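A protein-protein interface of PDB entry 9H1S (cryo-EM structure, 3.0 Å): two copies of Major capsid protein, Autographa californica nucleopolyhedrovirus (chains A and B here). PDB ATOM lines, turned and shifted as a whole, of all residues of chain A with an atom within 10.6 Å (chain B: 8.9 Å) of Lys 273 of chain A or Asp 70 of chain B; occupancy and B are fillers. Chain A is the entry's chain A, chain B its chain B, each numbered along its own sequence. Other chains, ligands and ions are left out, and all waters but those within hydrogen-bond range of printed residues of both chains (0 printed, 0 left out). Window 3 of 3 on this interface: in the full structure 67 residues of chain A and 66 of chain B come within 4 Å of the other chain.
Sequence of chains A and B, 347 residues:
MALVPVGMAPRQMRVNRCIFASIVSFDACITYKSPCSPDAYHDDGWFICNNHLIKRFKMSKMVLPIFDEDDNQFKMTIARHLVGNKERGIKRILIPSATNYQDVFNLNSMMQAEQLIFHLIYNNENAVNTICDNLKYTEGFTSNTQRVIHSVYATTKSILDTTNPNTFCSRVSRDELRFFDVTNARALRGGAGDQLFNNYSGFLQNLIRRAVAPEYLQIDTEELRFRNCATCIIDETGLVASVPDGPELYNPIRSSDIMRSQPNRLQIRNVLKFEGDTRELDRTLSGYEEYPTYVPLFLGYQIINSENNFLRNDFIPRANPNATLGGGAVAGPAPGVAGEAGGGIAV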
ATOM      1  N   LYS A  86     -17.134  -3.704  31.501  1.00  0.00           N
ATOM      2  CA  LYS A  86     -18.480  -3.176  31.607  1.00  0.00           C
ATOM      3  C   LYS A  86     -19.551  -4.094  31.025  1.00  0.00           C
ATOM      4  O   LYS A  86     -20.734  -3.759  31.062  1.00  0.00           O
ATOM      5  CB  LYS A  86     -18.535  -1.833  30.901  1.00  0.00           C
ATOM      6  CG  LYS A  86     -17.492  -0.843  31.396  1.00  0.00           C
ATOM      7  CD  LYS A  86     -17.641  -0.521  32.872  1.00  0.00           C
ATOM      8  CE  LYS A  86     -16.585   0.495  33.291  1.00  0.00           C
ATOM      9  NZ  LYS A  86     -16.633   0.801  34.745  1.00  0.00           N
ATOM     10  N   TYR A 250     -10.592  -5.695  35.215  1.00  0.00           N
ATOM     11  CA  TYR A 250     -10.378  -4.790  34.117  1.00  0.00           C
ATOM     12  C   TYR A 250      -9.799  -5.536  32.951  1.00  0.00           C
ATOM     13  O   TYR A 250      -8.818  -6.261  33.097  1.00  0.00           O
ATOM     14  CB  TYR A 250      -9.466  -3.647  34.511  1.00  0.00           C
ATOM     15  CG  TYR A 250      -9.151  -2.754  33.344  1.00  0.00           C
ATOM     16  CD1 TYR A 250     -10.176  -2.158  32.637  1.00  0.00           C
ATOM     17  CD2 TYR A 250      -7.836  -2.522  32.986  1.00  0.00           C
ATOM     18  CE1 TYR A 250      -9.887  -1.336  31.573  1.00  0.00           C
ATOM     19  CE2 TYR A 250      -7.547  -1.694  31.923  1.00  0.00           C
ATOM     20  CZ  TYR A 250      -8.569  -1.102  31.220  1.00  0.00           C
ATOM     21  OH  TYR A 250      -8.294  -0.272  30.161  1.00  0.00           O
ATOM     22  N   ASN A 251     -10.399  -5.365  31.792  1.00  0.00           N
ATOM     23  CA  ASN A 251      -9.905  -6.047  30.626  1.00  0.00           C
ATOM     24  C   ASN A 251     -10.063  -5.140  29.411  1.00  0.00           C
ATOM     25  O   ASN A 251     -11.167  -5.007  28.887  1.00  0.00           O
ATOM     26  CB  ASN A 251     -10.634  -7.344  30.430  1.00  0.00           C
ATOM     27  CG  ASN A 251     -10.021  -8.195  29.360  1.00  0.00           C
ATOM     28  OD1 ASN A 251      -8.898  -7.940  28.911  1.00  0.00           O
ATOM     29  ND2 ASN A 251     -10.734  -9.209  28.947  1.00  0.00           N
ATOM     30  N   PRO A 252      -8.988  -4.491  28.970  1.00  0.00           N
ATOM     31  CA  PRO A 252      -8.899  -3.562  27.866  1.00  0.00           C
ATOM     32  C   PRO A 252      -9.039  -4.272  26.545  1.00  0.00           C
ATOM     33  O   PRO A 252      -8.086  -4.877  26.049  1.00  0.00           O
ATOM     34  CB  PRO A 252      -7.517  -2.947  28.014  1.00  0.00           C
ATOM     35  CG  PRO A 252      -6.708  -3.988  28.695  1.00  0.00           C
ATOM     36  CD  PRO A 252      -7.672  -4.727  29.583  1.00  0.00           C
ATOM     37  N   ILE A 253     -10.225  -4.212  25.954  1.00  0.00           N
ATOM     38  CA  ILE A 253     -10.426  -4.917  24.704  1.00  0.00           C
ATOM     39  C   ILE A 253      -9.988  -4.050  23.554  1.00  0.00           C
ATOM     40  O   ILE A 253     -10.784  -3.364  22.915  1.00  0.00           O
ATOM     41  CB  ILE A 253     -11.877  -5.331  24.532  1.00  0.00           C
ATOM     42  CG1 ILE A 253     -12.324  -6.069  25.782  1.00  0.00           C
ATOM     43  CG2 ILE A 253     -12.021  -6.224  23.314  1.00  0.00           C
ATOM     44  CD1 ILE A 253     -11.457  -7.258  26.087  1.00  0.00           C
ATOM     45  N   ARG A 254      -8.695  -4.095  23.319  1.00  0.00           N
ATOM     46  CA  ARG A 254      -8.024  -3.325  22.299  1.00  0.00           C
ATOM     47  C   ARG A 254      -8.105  -3.942  20.934  1.00  0.00           C
ATOM     48  O   ARG A 254      -8.468  -5.105  20.792  1.00  0.00           O
ATOM     49  CB  ARG A 254      -6.592  -3.163  22.683  1.00  0.00           C
ATOM     50  CG  ARG A 254      -6.421  -2.355  23.933  1.00  0.00           C
ATOM     51  CD  ARG A 254      -5.036  -2.387  24.406  1.00  0.00           C
ATOM     52  NE  ARG A 254      -4.109  -1.784  23.467  1.00  0.00           N
ATOM     53  CZ  ARG A 254      -3.821  -0.471  23.392  1.00  0.00           C
ATOM     54  NH1 ARG A 254      -4.419   0.397  24.180  1.00  0.00           N
ATOM     55  NH2 ARG A 254      -2.919  -0.064  22.515  1.00  0.00           N
ATOM     56  N   SER A 255      -7.763  -3.147  19.929  1.00  0.00           N
ATOM     57  CA  SER A 255      -7.752  -3.599  18.550  1.00  0.00           C
ATOM     58  C   SER A 255      -6.581  -4.536  18.310  1.00  0.00           C
ATOM     59  O   SER A 255      -5.740  -4.737  19.187  1.00  0.00           O
ATOM     60  CB  SER A 255      -7.671  -2.425  17.605  1.00  0.00           C
ATOM     61  OG  SER A 255      -6.415  -1.810  17.678  1.00  0.00           O
ATOM     62  N   SER A 256      -6.551  -5.111  17.107  1.00  0.00           N
ATOM     63  CA  SER A 256      -5.574  -6.109  16.641  1.00  0.00           C
ATOM     64  C   SER A 256      -6.080  -7.524  16.923  1.00  0.00           C
ATOM     65  O   SER A 256      -5.488  -8.505  16.470  1.00  0.00           O
ATOM     66  CB  SER A 256      -4.201  -5.932  17.276  1.00  0.00           C
ATOM     67  OG  SER A 256      -4.122  -6.557  18.528  1.00  0.00           O
ATOM     68  N   ILE A 258      -9.703  -7.503  17.041  1.00  0.00           N
ATOM     69  CA  ILE A 258     -11.060  -7.050  16.776  1.00  0.00           C
ATOM     70  C   ILE A 258     -11.228  -6.865  15.283  1.00  0.00           C
ATOM     71  O   ILE A 258     -10.413  -6.195  14.648  1.00  0.00           O
ATOM     72  CB  ILE A 258     -11.382  -5.709  17.456  1.00  0.00           C
ATOM     73  CG1 ILE A 258     -11.234  -5.806  18.966  1.00  0.00           C
ATOM     74  CG2 ILE A 258     -12.791  -5.268  17.095  1.00  0.00           C
ATOM     75  CD1 ILE A 258     -11.388  -4.466  19.644  1.00  0.00           C
ATOM     76  N   ARG A 260     -14.020  -5.900  12.054  1.00  0.00           N
ATOM     77  CA  ARG A 260     -15.312  -5.463  11.535  1.00  0.00           C
ATOM     78  C   ARG A 260     -15.777  -6.410  10.443  1.00  0.00           C
ATOM     79  O   ARG A 260     -15.775  -6.072   9.259  1.00  0.00           O
ATOM     80  CB  ARG A 260     -15.244  -4.038  10.989  1.00  0.00           C
ATOM     81  CG  ARG A 260     -15.031  -2.939  12.026  1.00  0.00           C
ATOM     82  CD  ARG A 260     -14.946  -1.593  11.388  1.00  0.00           C
ATOM     83  NE  ARG A 260     -14.906  -0.514  12.371  1.00  0.00           N
ATOM     84  CZ  ARG A 260     -14.833   0.802  12.071  1.00  0.00           C
ATOM     85  NH1 ARG A 260     -14.758   1.188  10.816  1.00  0.00           N
ATOM     86  NH2 ARG A 260     -14.842   1.700  13.044  1.00  0.00           N
ATOM     87  N   ARG A 269     -19.889   1.118  20.987  1.00  0.00           N
ATOM     88  CA  ARG A 269     -19.109   0.603  22.097  1.00  0.00           C
ATOM     89  C   ARG A 269     -18.648   1.646  23.110  1.00  0.00           C
ATOM     90  O   ARG A 269     -18.293   2.768  22.755  1.00  0.00           O
ATOM     91  CB  ARG A 269     -17.878  -0.118  21.584  1.00  0.00           C
ATOM     92  CG  ARG A 269     -17.038  -0.687  22.701  1.00  0.00           C
ATOM     93  CD  ARG A 269     -15.927  -1.544  22.256  1.00  0.00           C
ATOM     94  NE  ARG A 269     -15.160  -1.967  23.414  1.00  0.00           N
ATOM     95  CZ  ARG A 269     -15.465  -3.042  24.164  1.00  0.00           C
ATOM     96  NH1 ARG A 269     -16.495  -3.791  23.829  1.00  0.00           N
ATOM     97  NH2 ARG A 269     -14.752  -3.349  25.236  1.00  0.00           N
ATOM     98  N   ASN A 270     -18.659   1.251  24.385  1.00  0.00           N
ATOM     99  CA  ASN A 270     -18.142   2.078  25.470  1.00  0.00           C
ATOM    100  C   ASN A 270     -16.654   1.806  25.591  1.00  0.00           C
ATOM    101  O   ASN A 270     -16.243   0.671  25.821  1.00  0.00           O
ATOM    102  CB  ASN A 270     -18.836   1.780  26.777  1.00  0.00           C
ATOM    103  CG  ASN A 270     -20.282   2.150  26.762  1.00  0.00           C
ATOM    104  OD1 ASN A 270     -20.658   3.237  26.314  1.00  0.00           O
ATOM    105  ND2 ASN A 270     -21.111   1.264  27.248  1.00  0.00           N
ATOM    106  N   VAL A 271     -15.854   2.837  25.405  1.00  0.00           N
ATOM    107  CA  VAL A 271     -14.412   2.711  25.380  1.00  0.00           C
ATOM    108  C   VAL A 271     -13.699   3.495  26.464  1.00  0.00           C
ATOM    109  O   VAL A 271     -13.933   4.687  26.655  1.00  0.00           O
ATOM    110  CB  VAL A 271     -13.907   3.170  24.012  1.00  0.00           C
ATOM    111  CG1 VAL A 271     -12.398   3.139  23.954  1.00  0.00           C
ATOM    112  CG2 VAL A 271     -14.484   2.269  22.946  1.00  0.00           C
ATOM    113  N   LEU A 272     -12.805   2.830  27.174  1.00  0.00           N
ATOM    114  CA  LEU A 272     -12.037   3.526  28.191  1.00  0.00           C
ATOM    115  C   LEU A 272     -10.820   4.198  27.565  1.00  0.00           C
ATOM    116  O   LEU A 272      -9.990   3.538  26.948  1.00  0.00           O
ATOM    117  CB  LEU A 272     -11.610   2.557  29.285  1.00  0.00           C
ATOM    118  CG  LEU A 272     -10.989   3.215  30.510  1.00  0.00           C
ATOM    119  CD1 LEU A 272     -11.182   2.326  31.725  1.00  0.00           C
ATOM    120  CD2 LEU A 272      -9.508   3.446  30.263  1.00  0.00           C
ATOM    121  N   LYS A 273     -10.723   5.517  27.710  1.00  0.00           N
ATOM    122  CA  LYS A 273      -9.618   6.288  27.146  1.00  0.00           C
ATOM    123  C   LYS A 273      -8.693   6.951  28.168  1.00  0.00           C
ATOM    124  O   LYS A 273      -9.145   7.659  29.064  1.00  0.00           O
ATOM    125  CB  LYS A 273     -10.176   7.363  26.234  1.00  0.00           C
ATOM    126  CG  LYS A 273      -9.120   8.225  25.572  1.00  0.00           C
ATOM    127  CD  LYS A 273      -9.756   9.248  24.651  1.00  0.00           C
ATOM    128  CE  LYS A 273     -10.267   8.589  23.385  1.00  0.00           C
ATOM    129  NZ  LYS A 273      -9.143   8.157  22.517  1.00  0.00           N
ATOM    130  N   PHE A 274      -7.383   6.745  28.018  1.00  0.00           N
ATOM    131  CA  PHE A 274      -6.414   7.424  28.883  1.00  0.00           C
ATOM    132  C   PHE A 274      -6.005   8.785  28.353  1.00  0.00           C
ATOM    133  O   PHE A 274      -5.765   8.952  27.157  1.00  0.00           O
ATOM    134  CB  PHE A 274      -5.117   6.638  29.044  1.00  0.00           C
ATOM    135  CG  PHE A 274      -5.185   5.421  29.891  1.00  0.00           C
ATOM    136  CD1 PHE A 274      -6.198   5.258  30.814  1.00  0.00           C
ATOM    137  CD2 PHE A 274      -4.217   4.435  29.769  1.00  0.00           C
ATOM    138  CE1 PHE A 274      -6.250   4.127  31.599  1.00  0.00           C
ATOM    139  CE2 PHE A 274      -4.269   3.302  30.551  1.00  0.00           C
ATOM    140  CZ  PHE A 274      -5.290   3.150  31.466  1.00  0.00           C
ATOM    141  N   GLU A 275      -5.861   9.737  29.266  1.00  0.00           N
ATOM    142  CA  GLU A 275      -5.360  11.056  28.943  1.00  0.00           C
ATOM    143  C   GLU A 275      -4.130  11.369  29.767  1.00  0.00           C
ATOM    144  O   GLU A 275      -3.968  10.884  30.889  1.00  0.00           O
ATOM    145  CB  GLU A 275      -6.414  12.116  29.163  1.00  0.00           C
ATOM    146  CG  GLU A 275      -7.597  12.017  28.228  1.00  0.00           C
ATOM    147  CD  GLU A 275      -7.199  12.300  26.808  1.00  0.00           C
ATOM    148  OE1 GLU A 275      -6.057  12.627  26.590  1.00  0.00           O
ATOM    149  OE2 GLU A 275      -8.043  12.239  25.944  1.00  0.00           O
ATOM    150  N   GLY A 276      -3.279  12.205  29.200  1.00  0.00           N
ATOM    151  CA  GLY A 276      -2.011  12.578  29.797  1.00  0.00           C
ATOM    152  C   GLY A 276      -0.900  11.997  28.940  1.00  0.00           C
ATOM    153  O   GLY A 276      -1.126  11.051  28.186  1.00  0.00           O
ATOM    154  N   THR A 278       1.928   9.790  28.650  1.00  0.00           N
ATOM    155  CA  THR A 278       2.543   8.678  29.343  1.00  0.00           C
ATOM    156  C   THR A 278       3.831   8.209  28.699  1.00  0.00           C
ATOM    157  O   THR A 278       4.437   7.254  29.178  1.00  0.00           O
ATOM    158  CB  THR A 278       1.595   7.472  29.373  1.00  0.00           C
ATOM    159  OG1 THR A 278       1.351   7.042  28.029  1.00  0.00           O
ATOM    160  CG2 THR A 278       0.268   7.827  30.020  1.00  0.00           C
ATOM    161  N   PHE B  67      -3.036  -0.893  29.717  1.00  0.00           N
ATOM    162  CA  PHE B  67      -3.532  -0.247  28.532  1.00  0.00           C
ATOM    163  C   PHE B  67      -4.964   0.161  28.636  1.00  0.00           C
ATOM    164  O   PHE B  67      -5.753  -0.475  29.338  1.00  0.00           O
ATOM    165  CB  PHE B  67      -3.430  -1.142  27.334  1.00  0.00           C
ATOM    166  CG  PHE B  67      -2.066  -1.500  26.880  1.00  0.00           C
ATOM    167  CD1 PHE B  67      -1.378  -0.665  26.025  1.00  0.00           C
ATOM    168  CD2 PHE B  67      -1.477  -2.677  27.282  1.00  0.00           C
ATOM    169  CE1 PHE B  67      -0.123  -1.003  25.576  1.00  0.00           C
ATOM    170  CE2 PHE B  67      -0.219  -3.018  26.839  1.00  0.00           C
ATOM    171  CZ  PHE B  67       0.458  -2.181  25.985  1.00  0.00           C
ATOM    172  N   ASP B  68      -5.299   1.211  27.906  1.00  0.00           N
ATOM    173  CA  ASP B  68      -6.676   1.612  27.766  1.00  0.00           C
ATOM    174  C   ASP B  68      -7.218   0.888  26.563  1.00  0.00           C
ATOM    175  O   ASP B  68      -6.541   0.036  25.993  1.00  0.00           O
ATOM    176  CB  ASP B  68      -6.840   3.102  27.598  1.00  0.00           C
ATOM    177  CG  ASP B  68      -6.298   3.633  26.303  1.00  0.00           C
ATOM    178  OD1 ASP B  68      -5.841   2.852  25.494  1.00  0.00           O
ATOM    179  OD2 ASP B  68      -6.410   4.819  26.098  1.00  0.00           O
ATOM    180  N   GLU B  69      -8.415   1.234  26.143  1.00  0.00           N
ATOM    181  CA  GLU B  69      -9.005   0.582  25.003  1.00  0.00           C
ATOM    182  C   GLU B  69      -8.895   1.406  23.731  1.00  0.00           C
ATOM    183  O   GLU B  69      -9.725   1.266  22.833  1.00  0.00           O
ATOM    184  CB  GLU B  69     -10.451   0.292  25.304  1.00  0.00           C
ATOM    185  CG  GLU B  69     -10.642  -0.661  26.449  1.00  0.00           C
ATOM    186  CD  GLU B  69     -12.071  -1.028  26.646  1.00  0.00           C
ATOM    187  OE1 GLU B  69     -12.881  -0.146  26.818  1.00  0.00           O
ATOM    188  OE2 GLU B  69     -12.359  -2.205  26.604  1.00  0.00           O
ATOM    189  N   ASP B  70      -7.887   2.267  23.645  1.00  0.00           N
ATOM    190  CA  ASP B  70      -7.745   3.110  22.477  1.00  0.00           C
ATOM    191  C   ASP B  70      -6.361   3.722  22.338  1.00  0.00           C
ATOM    192  O   ASP B  70      -6.197   4.939  22.424  1.00  0.00           O
ATOM    193  CB  ASP B  70      -8.777   4.227  22.491  1.00  0.00           C
ATOM    194  CG  ASP B  70      -8.787   4.991  21.176  1.00  0.00           C
ATOM    195  OD1 ASP B  70      -8.156   4.541  20.250  1.00  0.00           O
ATOM    196  OD2 ASP B  70      -9.415   6.021  21.109  1.00  0.00           O
ATOM    197  N   ASP B  71      -5.385   2.870  22.085  1.00  0.00           N
ATOM    198  CA  ASP B  71      -4.012   3.261  21.796  1.00  0.00           C
ATOM    199  C   ASP B  71      -3.207   4.011  22.865  1.00  0.00           C
ATOM    200  O   ASP B  71      -2.273   4.730  22.509  1.00  0.00           O
ATOM    201  CB  ASP B  71      -3.990   4.110  20.532  1.00  0.00           C
ATOM    202  CG  ASP B  71      -2.612   4.136  19.896  1.00  0.00           C
ATOM    203  OD1 ASP B  71      -1.891   3.182  20.074  1.00  0.00           O
ATOM    204  OD2 ASP B  71      -2.291   5.098  19.241  1.00  0.00           O
ATOM    205  N   ASN B  72      -3.484   3.814  24.154  1.00  0.00           N
ATOM    206  CA  ASN B  72      -2.601   4.442  25.136  1.00  0.00           C
ATOM    207  C   ASN B  72      -2.051   3.429  26.118  1.00  0.00           C
ATOM    208  O   ASN B  72      -2.766   2.583  26.662  1.00  0.00           O
ATOM    209  CB  ASN B  72      -3.277   5.555  25.883  1.00  0.00           C
ATOM    210  CG  ASN B  72      -3.684   6.684  24.993  1.00  0.00           C
ATOM    211  OD1 ASN B  72      -2.856   7.505  24.580  1.00  0.00           O
ATOM    212  ND2 ASN B  72      -4.951   6.739  24.682  1.00  0.00           N
ATOM    213  N   GLN B  73      -0.751   3.545  26.341  1.00  0.00           N
ATOM    214  CA  GLN B  73      -0.016   2.680  27.235  1.00  0.00           C
ATOM    215  C   GLN B  73       0.311   3.388  28.530  1.00  0.00           C
ATOM    216  O   GLN B  73       0.595   4.584  28.555  1.00  0.00           O
ATOM    217  CB  GLN B  73       1.254   2.190  26.568  1.00  0.00           C
ATOM    218  CG  GLN B  73       2.047   1.199  27.394  1.00  0.00           C
ATOM    219  CD  GLN B  73       3.203   0.629  26.607  1.00  0.00           C
ATOM    220  OE1 GLN B  73       3.722   1.263  25.684  1.00  0.00           O
ATOM    221  NE2 GLN B  73       3.609  -0.584  26.955  1.00  0.00           N
ATOM    222  N   ILE B 219      -9.058   5.631  39.484  1.00  0.00           N
ATOM    223  CA  ILE B 219      -8.587   6.875  38.913  1.00  0.00           C
ATOM    224  C   ILE B 219      -9.753   7.761  38.624  1.00  0.00           C
ATOM    225  O   ILE B 219     -10.550   7.460  37.739  1.00  0.00           O
ATOM    226  CB  ILE B 219      -7.816   6.634  37.622  1.00  0.00           C
ATOM    227  CG1 ILE B 219      -6.620   5.741  37.887  1.00  0.00           C
ATOM    228  CG2 ILE B 219      -7.377   7.956  37.012  1.00  0.00           C
ATOM    229  CD1 ILE B 219      -5.955   5.261  36.625  1.00  0.00           C
ATOM    230  N   GLU B 222     -12.991   6.044  38.528  1.00  0.00           N
ATOM    231  CA  GLU B 222     -13.049   4.868  37.682  1.00  0.00           C
ATOM    232  C   GLU B 222     -12.240   3.750  38.293  1.00  0.00           C
ATOM    233  O   GLU B 222     -11.010   3.774  38.273  1.00  0.00           O
ATOM    234  CB  GLU B 222     -12.542   5.170  36.282  1.00  0.00           C
ATOM    235  CG  GLU B 222     -12.612   3.973  35.354  1.00  0.00           C
ATOM    236  CD  GLU B 222     -14.027   3.529  35.101  1.00  0.00           C
ATOM    237  OE1 GLU B 222     -14.832   4.348  34.729  1.00  0.00           O
ATOM    238  OE2 GLU B 222     -14.308   2.369  35.290  1.00  0.00           O
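Among the printed residues, 24 pairs touch across the chains.
Among the printed residues, Asp or Glu carboxylates within 4 Å of a Lys or Arg side-chain nitrogen of the other chain: Lys 86 of chain A with Glu 222 of chain B (2.9 Å), Arg 254 of chain A with Asp 68 of chain B (3.1 Å), Arg 269 of chain A with Glu 69 of chain B (3.0 Å) and Lys 273 of chain A with Asp 70 of chain B (2.6 Å).
O of Phe 274 of chain A is in hydrogen-bond range of ND2 of Asn 72 of chain B, 3.4 Å away.
The backbone NH (N) of Ile 253 of chain A lies within hydrogen-bond range of the side-chain carboxylate (OE2) of Glu 69 of chain B, at 3.0 Å.
The guanidinium group of Arg 269 of chain A is in salt-bridge range of the side-chain carboxylate of Glu 69 of chain B, at 3.0 Å.
The guanidinium group (NH1) of Arg 254 of chain A sits close to the backbone NH (N) of Asp 71 of chain B (3.4 Å).
The side-chain amino group (NZ) of Lys 273 of chain A is in salt-bridge range of the side-chain carboxylate (OD2) of Asp 70 of chain B, 2.6 Å away.
NH1 of Arg 254 of chain A is in salt-bridge range of OD1 of Asp 68 of chain B, at 3.1 Å.
The side-chain hydroxyl of Tyr 250 of chain A sits at hydrogen-bond distance from the backbone carbonyl oxygen of Phe 67 of chain B, 2.7 Å away.
The backbone carbonyl oxygen of Leu 272 of chain A lies within hydrogen-bond range of the backbone NH of Glu 69 of chain B.
The backbone NH (N) of Phe 274 of chain A sits at hydrogen-bond distance from the side-chain carboxylate (OD2) of Asp 68 of chain B, 2.9 Å away.
The side-chain carboxylate of Glu 222 of chain B lies within salt-bridge range of the side-chain amino group of Lys 86 of chain A, 2.9 Å away.
O of Gln 73 of chain B lies within hydrogen-bond range of OG1 of Thr 278 of chain A, 2.6 Å away.
No position is printed for both chains.
Of the 24 pairs that touch across the chains among the printed residues, none has its exchanged pair printed and touching as well.
Printed residues of chain B within 4 Å of Arg 254 of chain A: Phe 67 (3.6 Å), Asp 68 (2.8 Å), Asp 70 (3.98 Å), Asp 71 (3.4 Å) and Asn 72 (3.5 Å).
Ser 256 of chain A touches none of the printed residues of chain B.
Ile 258 of chain A touches none of the printed residues of chain B.
Of the printed residues of chain B, Val 271 of chain A touches Glu 69 (3.5 Å).
Of chain B, only Asp 68 and Asp 70 come within 4 Å of Lys 273 of chain A.
Asp 71 of chain B touches one residue of chain A.
Of chain A, only Arg 254 (3.5 Å) and Phe 274 (3.4 Å) come within 4 Å of Asn 72 of chain B.
The nearest residue of chain A that does not touch Asp 70 of chain B is Val 271 of chain A (4.1 Å).
The nearest printed residue of chain B that does not touch Pro 252 of chain A is Asp 70 of chain B (6.8 Å).
N of Asp 71 of chain B is in hydrogen-bond range of OD1 of Asp 68 of chain B (3.4 Å).
The side-chain amide nitrogen of Asn 72 of chain B lies within hydrogen-bond range of the side-chain carboxylate of Asp 68 of chain B (2.8 Å).
ND2 of Asn 72 of chain B lies within hydrogen-bond range of O of Asp 70 of chain B (3.1 Å).
The backbone NH (N) of Asp 70 of chain B is in hydrogen-bond range of the side-chain carboxylate (OD1) of Asp 68 of chain B (2.8 Å).
Among the printed residues, pairs that only touch across the chains: Leu 272 of chain A with Asp 68 of chain B, Pro 252 of chain A with Phe 67 of chain B, Tyr 250 of chain A with Asp 68 of chain B, Val 271 of chain A with Glu 69 of chain B, Arg 254 of chain A with Asn 72 of chain B, Arg 254 of chain A with Phe 67 of chain B, Asn 270 of chain A with Glu 69 of chain B, Pro 252 of chain A with Glu 69 of chain B, Lys 273 of chain A with Asp 68 of chain B, Pro 252 of chain A with Asp 68 of chain B, Phe 274 of chain A with Phe 67 of chain B, Asn 251 of chain A with Glu 69 of chain B and Arg 254 of chain A with Asp 70 of chain B.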
